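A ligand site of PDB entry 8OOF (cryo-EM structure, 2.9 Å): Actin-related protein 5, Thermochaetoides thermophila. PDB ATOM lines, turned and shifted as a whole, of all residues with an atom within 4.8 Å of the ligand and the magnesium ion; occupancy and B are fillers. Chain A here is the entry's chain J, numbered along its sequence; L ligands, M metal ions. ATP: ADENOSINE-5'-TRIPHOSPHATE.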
ATOM      1  N   ASP A  62       6.662  -9.940 -17.618  1.00  0.00           N
ATOM      2  CA  ASP A  62       6.270  -8.621 -18.116  1.00  0.00           C
ATOM      3  C   ASP A  62       6.434  -8.590 -19.634  1.00  0.00           C
ATOM      4  O   ASP A  62       7.552  -8.632 -20.142  1.00  0.00           O
ATOM      5  CB  ASP A  62       7.100  -7.539 -17.428  1.00  0.00           C
ATOM      6  CG  ASP A  62       6.740  -6.140 -17.904  1.00  0.00           C
ATOM      7  OD1 ASP A  62       5.573  -5.924 -18.296  1.00  0.00           O
ATOM      8  OD2 ASP A  62       7.621  -5.262 -17.851  1.00  0.00           O
ATOM      9  N   ASN A  63       5.306  -8.524 -20.346  1.00  0.00           N
ATOM     10  CA  ASN A  63       5.256  -8.418 -21.802  1.00  0.00           C
ATOM     11  C   ASN A  63       5.664  -7.051 -22.337  1.00  0.00           C
ATOM     12  O   ASN A  63       4.847  -6.367 -22.961  1.00  0.00           O
ATOM     13  CB  ASN A  63       3.853  -8.736 -22.334  1.00  0.00           C
ATOM     14  CG  ASN A  63       3.642 -10.206 -22.536  1.00  0.00           C
ATOM     15  OD1 ASN A  63       4.451 -10.884 -23.171  1.00  0.00           O
ATOM     16  ND2 ASN A  63       2.527 -10.716 -22.042  1.00  0.00           N
ATOM     17  N   GLY A  64       6.912  -6.644 -22.113  1.00  0.00           N
ATOM     18  CA  GLY A  64       7.400  -5.441 -22.732  1.00  0.00           C
ATOM     19  C   GLY A  64       7.588  -5.623 -24.224  1.00  0.00           C
ATOM     20  O   GLY A  64       8.307  -6.530 -24.664  1.00  0.00           O
ATOM     21  N   SER A  65       6.933  -4.775 -25.026  1.00  0.00           N
ATOM     22  CA  SER A  65       7.156  -4.733 -26.464  1.00  0.00           C
ATOM     23  C   SER A  65       8.606  -4.454 -26.817  1.00  0.00           C
ATOM     24  O   SER A  65       9.069  -4.841 -27.894  1.00  0.00           O
ATOM     25  CB  SER A  65       6.259  -3.681 -27.110  1.00  0.00           C
ATOM     26  OG  SER A  65       4.916  -3.839 -26.703  1.00  0.00           O
ATOM     27  N   HIS A  66       9.340  -3.789 -25.931  1.00  0.00           N
ATOM     28  CA  HIS A  66      10.787  -3.695 -26.058  1.00  0.00           C
ATOM     29  C   HIS A  66      11.525  -4.845 -25.394  1.00  0.00           C
ATOM     30  O   HIS A  66      12.569  -5.273 -25.894  1.00  0.00           O
ATOM     31  CB  HIS A  66      11.254  -2.350 -25.479  1.00  0.00           C
ATOM     32  CG  HIS A  66      12.738  -2.202 -25.424  1.00  0.00           C
ATOM     33  ND1 HIS A  66      13.517  -2.006 -26.546  1.00  0.00           N
ATOM     34  CD2 HIS A  66      13.594  -2.209 -24.371  1.00  0.00           C
ATOM     35  CE1 HIS A  66      14.786  -1.904 -26.182  1.00  0.00           C
ATOM     36  NE2 HIS A  66      14.856  -2.028 -24.876  1.00  0.00           N
ATOM     37  N   SER A  67      11.037  -5.353 -24.267  1.00  0.00           N
ATOM     38  CA  SER A  67      11.734  -6.413 -23.548  1.00  0.00           C
ATOM     39  C   SER A  67      10.726  -7.254 -22.780  1.00  0.00           C
ATOM     40  O   SER A  67      10.064  -6.754 -21.875  1.00  0.00           O
ATOM     41  CB  SER A  67      12.780  -5.824 -22.603  1.00  0.00           C
ATOM     42  OG  SER A  67      13.556  -6.844 -22.009  1.00  0.00           O
ATOM     43  N   ARG A  69      10.378  -9.478 -19.881  1.00  0.00           N
ATOM     44  CA  ARG A  69      11.084  -9.717 -18.629  1.00  0.00           C
ATOM     45  C   ARG A  69      10.385 -10.819 -17.850  1.00  0.00           C
ATOM     46  O   ARG A  69       9.174 -10.747 -17.612  1.00  0.00           O
ATOM     47  CB  ARG A  69      11.153  -8.423 -17.813  1.00  0.00           C
ATOM     48  CG  ARG A  69      12.042  -7.384 -18.469  1.00  0.00           C
ATOM     49  CD  ARG A  69      11.710  -5.997 -17.993  1.00  0.00           C
ATOM     50  NE  ARG A  69      10.417  -5.591 -18.538  1.00  0.00           N
ATOM     51  CZ  ARG A  69      10.241  -4.552 -19.343  1.00  0.00           C
ATOM     52  NH1 ARG A  69      11.257  -3.808 -19.733  1.00  0.00           N
ATOM     53  NH2 ARG A  69       9.020  -4.275 -19.776  1.00  0.00           N
ATOM     54  N   GLY A 124       0.983  -1.736 -28.200  1.00  0.00           N
ATOM     55  CA  GLY A 124       1.251  -2.559 -27.044  1.00  0.00           C
ATOM     56  C   GLY A 124       0.630  -3.933 -27.115  1.00  0.00           C
ATOM     57  O   GLY A 124       0.689  -4.683 -26.132  1.00  0.00           O
ATOM     58  N   ASP A 190       1.293  -3.056 -16.365  1.00  0.00           N
ATOM     59  CA  ASP A 190       2.685  -2.862 -15.973  1.00  0.00           C
ATOM     60  C   ASP A 190       2.894  -1.559 -15.197  1.00  0.00           C
ATOM     61  O   ASP A 190       3.646  -1.525 -14.220  1.00  0.00           O
ATOM     62  CB  ASP A 190       3.588  -2.916 -17.206  1.00  0.00           C
ATOM     63  CG  ASP A 190       3.366  -1.743 -18.155  1.00  0.00           C
ATOM     64  OD1 ASP A 190       2.302  -1.085 -18.070  1.00  0.00           O
ATOM     65  OD2 ASP A 190       4.245  -1.493 -18.998  1.00  0.00           O
ATOM     66  N   SER A 208       5.550   6.372 -19.948  1.00  0.00           N
ATOM     67  CA  SER A 208       5.989   6.375 -21.333  1.00  0.00           C
ATOM     68  C   SER A 208       6.855   5.157 -21.564  1.00  0.00           C
ATOM     69  O   SER A 208       7.886   4.972 -20.908  1.00  0.00           O
ATOM     70  CB  SER A 208       6.760   7.650 -21.683  1.00  0.00           C
ATOM     71  OG  SER A 208       5.936   8.796 -21.546  1.00  0.00           O
ATOM     72  N   SER A 209       6.427   4.318 -22.514  1.00  0.00           N
ATOM     73  CA  SER A 209       7.065   3.041 -22.777  1.00  0.00           C
ATOM     74  C   SER A 209       7.408   2.944 -24.256  1.00  0.00           C
ATOM     75  O   SER A 209       7.398   3.957 -24.956  1.00  0.00           O
ATOM     76  CB  SER A 209       6.152   1.896 -22.334  1.00  0.00           C
ATOM     77  OG  SER A 209       4.990   1.831 -23.132  1.00  0.00           O
ATOM     78  N   TYR A 210       7.726   1.748 -24.727  1.00  0.00           N
ATOM     79  CA  TYR A 210       7.957   1.548 -26.156  1.00  0.00           C
ATOM     80  C   TYR A 210       6.693   1.831 -26.958  1.00  0.00           C
ATOM     81  O   TYR A 210       6.730   2.525 -27.976  1.00  0.00           O
ATOM     82  CB  TYR A 210       8.435   0.114 -26.393  1.00  0.00           C
ATOM     83  CG  TYR A 210       9.346  -0.088 -27.571  1.00  0.00           C
ATOM     84  CD1 TYR A 210      10.562   0.557 -27.663  1.00  0.00           C
ATOM     85  CD2 TYR A 210       8.992  -0.957 -28.595  1.00  0.00           C
ATOM     86  CE1 TYR A 210      11.395   0.373 -28.737  1.00  0.00           C
ATOM     87  CE2 TYR A 210       9.821  -1.165 -29.673  1.00  0.00           C
ATOM     88  CZ  TYR A 210      11.021  -0.492 -29.738  1.00  0.00           C
ATOM     89  OH  TYR A 210      11.857  -0.719 -30.807  1.00  0.00           O
ATOM     90  N   SER A 211       5.563   1.281 -26.514  1.00  0.00           N
ATOM     91  CA  SER A 211       4.370   1.269 -27.353  1.00  0.00           C
ATOM     92  C   SER A 211       3.655   2.623 -27.381  1.00  0.00           C
ATOM     93  O   SER A 211       3.082   2.996 -28.411  1.00  0.00           O
ATOM     94  CB  SER A 211       3.411   0.188 -26.872  1.00  0.00           C
ATOM     95  OG  SER A 211       3.087   0.361 -25.498  1.00  0.00           O
ATOM     96  N   ALA A 212       3.635   3.335 -26.273  1.00  0.00           N
ATOM     97  CA  ALA A 212       2.626   4.360 -26.049  1.00  0.00           C
ATOM     98  C   ALA A 212       3.039   5.199 -24.861  1.00  0.00           C
ATOM     99  O   ALA A 212       4.067   4.945 -24.217  1.00  0.00           O
ATOM    100  CB  ALA A 212       1.235   3.748 -25.849  1.00  0.00           C
ATOM    101  N   GLY A 235       8.767   5.165 -27.030  1.00  0.00           N
ATOM    102  CA  GLY A 235      10.153   4.983 -27.395  1.00  0.00           C
ATOM    103  C   GLY A 235      10.359   4.387 -28.775  1.00  0.00           C
ATOM    104  O   GLY A 235      11.389   4.632 -29.414  1.00  0.00           O
ATOM    105  N   TRP A 236       9.404   3.595 -29.256  1.00  0.00           N
ATOM    106  CA  TRP A 236       9.472   3.086 -30.617  1.00  0.00           C
ATOM    107  C   TRP A 236       9.330   4.217 -31.623  1.00  0.00           C
ATOM    108  O   TRP A 236      10.128   4.351 -32.552  1.00  0.00           O
ATOM    109  CB  TRP A 236       8.377   2.048 -30.847  1.00  0.00           C
ATOM    110  CG  TRP A 236       8.410   1.447 -32.200  1.00  0.00           C
ATOM    111  CD1 TRP A 236       9.239   0.455 -32.636  1.00  0.00           C
ATOM    112  CD2 TRP A 236       7.615   1.821 -33.335  1.00  0.00           C
ATOM    113  NE1 TRP A 236       8.995   0.168 -33.946  1.00  0.00           N
ATOM    114  CE2 TRP A 236       7.998   0.994 -34.404  1.00  0.00           C
ATOM    115  CE3 TRP A 236       6.613   2.764 -33.537  1.00  0.00           C
ATOM    116  CZ2 TRP A 236       7.417   1.093 -35.662  1.00  0.00           C
ATOM    117  CZ3 TRP A 236       6.025   2.854 -34.785  1.00  0.00           C
ATOM    118  CH2 TRP A 236       6.435   2.015 -35.834  1.00  0.00           C
ATOM    119  N   GLU A 264      17.552   4.228 -32.031  1.00  0.00           N
ATOM    120  CA  GLU A 264      17.120   3.942 -30.665  1.00  0.00           C
ATOM    121  C   GLU A 264      18.224   4.185 -29.650  1.00  0.00           C
ATOM    122  O   GLU A 264      17.959   4.722 -28.565  1.00  0.00           O
ATOM    123  CB  GLU A 264      16.619   2.505 -30.578  1.00  0.00           C
ATOM    124  CG  GLU A 264      15.874   2.170 -29.326  1.00  0.00           C
ATOM    125  CD  GLU A 264      15.749   0.674 -29.124  1.00  0.00           C
ATOM    126  OE1 GLU A 264      14.911   0.053 -29.801  1.00  0.00           O
ATOM    127  OE2 GLU A 264      16.507   0.128 -28.299  1.00  0.00           O
ATOM    128  N   ARG A 268      18.437   7.351 -26.706  1.00  0.00           N
ATOM    129  CA  ARG A 268      18.885   7.142 -25.331  1.00  0.00           C
ATOM    130  C   ARG A 268      20.056   8.047 -24.967  1.00  0.00           C
ATOM    131  O   ARG A 268      19.999   8.773 -23.965  1.00  0.00           O
ATOM    132  CB  ARG A 268      19.255   5.681 -25.113  1.00  0.00           C
ATOM    133  CG  ARG A 268      18.090   4.728 -25.191  1.00  0.00           C
ATOM    134  CD  ARG A 268      18.530   3.324 -24.850  1.00  0.00           C
ATOM    135  NE  ARG A 268      17.731   2.320 -25.529  1.00  0.00           N
ATOM    136  CZ  ARG A 268      17.908   1.011 -25.417  1.00  0.00           C
ATOM    137  NH1 ARG A 268      18.726   0.507 -24.502  1.00  0.00           N
ATOM    138  NH2 ARG A 268      17.195   0.180 -26.175  1.00  0.00           N
ATOM    139  N   GLY A 690       8.151   3.718 -16.660  1.00  0.00           N
ATOM    140  CA  GLY A 690       8.567   3.291 -17.972  1.00  0.00           C
ATOM    141  C   GLY A 690       9.800   3.988 -18.508  1.00  0.00           C
ATOM    142  O   GLY A 690      10.100   5.137 -18.162  1.00  0.00           O
ATOM    143  N   GLY A 691      10.535   3.263 -19.360  1.00  0.00           N
ATOM    144  CA  GLY A 691      11.872   3.696 -19.754  1.00  0.00           C
ATOM    145  C   GLY A 691      11.883   5.004 -20.523  1.00  0.00           C
ATOM    146  O   GLY A 691      12.783   5.827 -20.350  1.00  0.00           O
ATOM    147  N   ASN A 692      10.895   5.217 -21.379  1.00  0.00           N
ATOM    148  CA  ASN A 692      10.838   6.417 -22.194  1.00  0.00           C
ATOM    149  C   ASN A 692      10.552   7.697 -21.400  1.00  0.00           C
ATOM    150  O   ASN A 692      10.472   8.773 -22.003  1.00  0.00           O
ATOM    151  CB  ASN A 692       9.782   6.196 -23.287  1.00  0.00           C
ATOM    152  CG  ASN A 692       9.711   7.335 -24.286  1.00  0.00           C
ATOM    153  OD1 ASN A 692       8.678   7.965 -24.465  1.00  0.00           O
ATOM    154  ND2 ASN A 692      10.829   7.587 -24.961  1.00  0.00           N
ATOM    155  N   LEU A 694      12.842   8.479 -19.071  1.00  0.00           N
ATOM    156  CA  LEU A 694      14.148   8.693 -18.468  1.00  0.00           C
ATOM    157  C   LEU A 694      14.936   9.839 -19.088  1.00  0.00           C
ATOM    158  O   LEU A 694      16.135   9.970 -18.808  1.00  0.00           O
ATOM    159  CB  LEU A 694      14.980   7.408 -18.529  1.00  0.00           C
ATOM    160  CG  LEU A 694      14.505   6.271 -17.619  1.00  0.00           C
ATOM    161  CD1 LEU A 694      15.220   4.986 -17.966  1.00  0.00           C
ATOM    162  CD2 LEU A 694      14.749   6.648 -16.164  1.00  0.00           C
ATOM    163  N   PHE A 695      14.317  10.656 -19.938  1.00  0.00           N
ATOM    164  CA  PHE A 695      15.002  11.834 -20.461  1.00  0.00           C
ATOM    165  C   PHE A 695      15.345  12.814 -19.338  1.00  0.00           C
ATOM    166  O   PHE A 695      14.585  12.985 -18.388  1.00  0.00           O
ATOM    167  CB  PHE A 695      14.135  12.523 -21.505  1.00  0.00           C
ATOM    168  CG  PHE A 695      13.875  11.692 -22.712  1.00  0.00           C
ATOM    169  CD1 PHE A 695      14.918  11.318 -23.534  1.00  0.00           C
ATOM    170  CD2 PHE A 695      12.601  11.268 -23.018  1.00  0.00           C
ATOM    171  CE1 PHE A 695      14.684  10.543 -24.643  1.00  0.00           C
ATOM    172  CE2 PHE A 695      12.364  10.499 -24.135  1.00  0.00           C
ATOM    173  CZ  PHE A 695      13.417  10.137 -24.938  1.00  0.00           C
ATOM    174  N   ILE A 725      12.540   1.015 -15.467  1.00  0.00           N
ATOM    175  CA  ILE A 725      12.301  -0.124 -16.355  1.00  0.00           C
ATOM    176  C   ILE A 725      11.890  -1.382 -15.570  1.00  0.00           C
ATOM    177  O   ILE A 725      10.797  -1.918 -15.774  1.00  0.00           O
ATOM    178  CB  ILE A 725      13.531  -0.375 -17.251  1.00  0.00           C
ATOM    179  CG1 ILE A 725      14.817  -0.403 -16.434  1.00  0.00           C
ATOM    180  CG2 ILE A 725      13.619   0.693 -18.330  1.00  0.00           C
ATOM    181  CD1 ILE A 725      15.903  -1.241 -17.061  1.00  0.00           C
HETATM  182  PG  ATP L   1       5.353  -1.697 -23.424  1.00  0.00           P
HETATM  183  O1G ATP L   1       4.834  -1.605 -22.031  1.00  0.00           O
HETATM  184  O2G ATP L   1       4.848  -2.919 -24.196  1.00  0.00           O
HETATM  185  O3G ATP L   1       5.097  -0.470 -24.256  1.00  0.00           O
HETATM  186  PB  ATP L   1       8.096  -2.000 -22.393  1.00  0.00           P
HETATM  187  O1B ATP L   1       7.599  -2.399 -21.065  1.00  0.00           O
HETATM  188  O2B ATP L   1       9.166  -2.886 -23.013  1.00  0.00           O
HETATM  189  O3B ATP L   1       6.923  -1.862 -23.412  1.00  0.00           O
HETATM  190  PA  ATP L   1       9.660   0.313 -21.482  1.00  0.00           P
HETATM  191  O1A ATP L   1       8.905   1.038 -20.442  1.00  0.00           O
HETATM  192  O2A ATP L   1      10.753  -0.614 -20.989  1.00  0.00           O
HETATM  193  O3A ATP L   1       8.693  -0.530 -22.384  1.00  0.00           O
HETATM  194  O5' ATP L   1      10.288   1.294 -22.547  1.00  0.00           O
HETATM  195  C5' ATP L   1      11.541   0.989 -23.194  1.00  0.00           C
HETATM  196  C4' ATP L   1      11.956   2.195 -23.994  1.00  0.00           C
HETATM  197  O4' ATP L   1      12.709   3.098 -23.155  1.00  0.00           O
HETATM  198  C3' ATP L   1      12.828   1.896 -25.207  1.00  0.00           C
HETATM  199  O3' ATP L   1      12.422   2.665 -26.331  1.00  0.00           O
HETATM  200  C2' ATP L   1      14.230   2.303 -24.736  1.00  0.00           C
HETATM  201  O2' ATP L   1      15.041   2.729 -25.812  1.00  0.00           O
HETATM  202  C1' ATP L   1      13.886   3.474 -23.823  1.00  0.00           C
HETATM  203  N9  ATP L   1      14.903   3.784 -22.831  1.00  0.00           N
HETATM  204  C8  ATP L   1      15.608   2.895 -22.064  1.00  0.00           C
HETATM  205  N7  ATP L   1      16.478   3.459 -21.260  1.00  0.00           N
HETATM  206  C5  ATP L   1      16.343   4.817 -21.518  1.00  0.00           C
HETATM  207  C6  ATP L   1      16.981   5.955 -20.995  1.00  0.00           C
HETATM  208  N6  ATP L   1      17.927   5.917 -20.059  1.00  0.00           N
HETATM  209  N1  ATP L   1      16.603   7.161 -21.479  1.00  0.00           N
HETATM  210  C2  ATP L   1      15.653   7.213 -22.416  1.00  0.00           C
HETATM  211  N3  ATP L   1      14.982   6.208 -22.983  1.00  0.00           N
HETATM  212  C4  ATP L   1      15.376   5.022 -22.489  1.00  0.00           C
HETATM  213 MG    MG M   1       5.887  -1.557 -20.213  1.00  0.00          MG
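Residues that only touch the ligand: Asn 63 (3.7 Å), Gly 64 (3.1 Å), Gly 235 (3.4 Å), Glu 264 (3.7 Å), Gly 690 (3.4 Å) and Leu 694 (3.4 Å).
Of the 24 residues printed, 17 come within 4 Å of the ligand.
Along chain A the residues within 4 Å of the ligand span positions 63 to 694.
The nearest printed residue that does not touch the ligand is Ser 208 (4.1 Å).
The side-chain hydroxyl of Ser 211 sits at hydrogen-bond distance from the side-chain hydroxyl of Ser 209, 3.4 Å away.
The guanidinium group (NH2) of Arg 69 lies close to the backbone carbonyl oxygen (O) of Ser 67, 3.4 Å away.
N of Gly 235 sits at hydrogen-bond distance from O of Tyr 210, at 3.5 Å.
OD2 of Asp 62 is in salt-bridge range of NH2 of Arg 69, at 2.6 Å.
O of Tyr 210 lies within hydrogen-bond range of N of Trp 236 (3.2 Å).
NE2 of His 66 sits close to NH2 of Arg 268 (3.5 Å).
The guanidinium group (NE) of Arg 268 is in salt-bridge range of the side-chain carboxylate (OE2) of Glu 264 (3.7 Å).
OE1 of Glu 264 lies within hydrogen-bond range of OH of Tyr 210.
The backbone NH of Tyr 210 is in hydrogen-bond range of an oxygen (O5') of the ligand (3.4 Å).
The side-chain hydroxyl (OG) of Ser 209 lies within hydrogen-bond range of an oxygen (O3G) of the ligand.
An oxygen (O3G) of the ligand is in hydrogen-bond range of the backbone NH of Ser 211 (2.9 Å).
N of Ser 65 lies within hydrogen-bond range of O2G of the ligand (2.9 Å).
The side-chain hydroxyl of Ser 211 sits at hydrogen-bond distance from an oxygen (O3G) of the ligand (2.5 Å).
The side-chain hydroxyl (OG) of Ser 65 is in hydrogen-bond range of an oxygen (O2G) of the ligand (2.7 Å).
The backbone NH (N) of Ser 67 sits at hydrogen-bond distance from an oxygen (O2B) of the ligand (3.3 Å).
N of His 66 is in hydrogen-bond range of O2B of the ligand (3.1 Å).
NE of Arg 268 sits at hydrogen-bond distance from O2' of the ligand (2.7 Å).
An oxygen (O2A) of the ligand lies within salt-bridge range of the guanidinium group (NH1) of Arg 69, 3.5 Å away.
The backbone NH of Gly 691 is in hydrogen-bond range of an oxygen (O1A) of the ligand, 3.0 Å away.
An oxygen (O4') of the ligand is in hydrogen-bond range of the backbone NH (N) of Asn 692, 3.3 Å away.
The nearest printed residue that does not touch the magnesium ion is Ser 209 (4.1 Å).
The magnesium ion is bound by the side-chain carboxylate of Asp 190, an oxygen (O1B) of the ligand and an oxygen (O1G) of the ligand.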
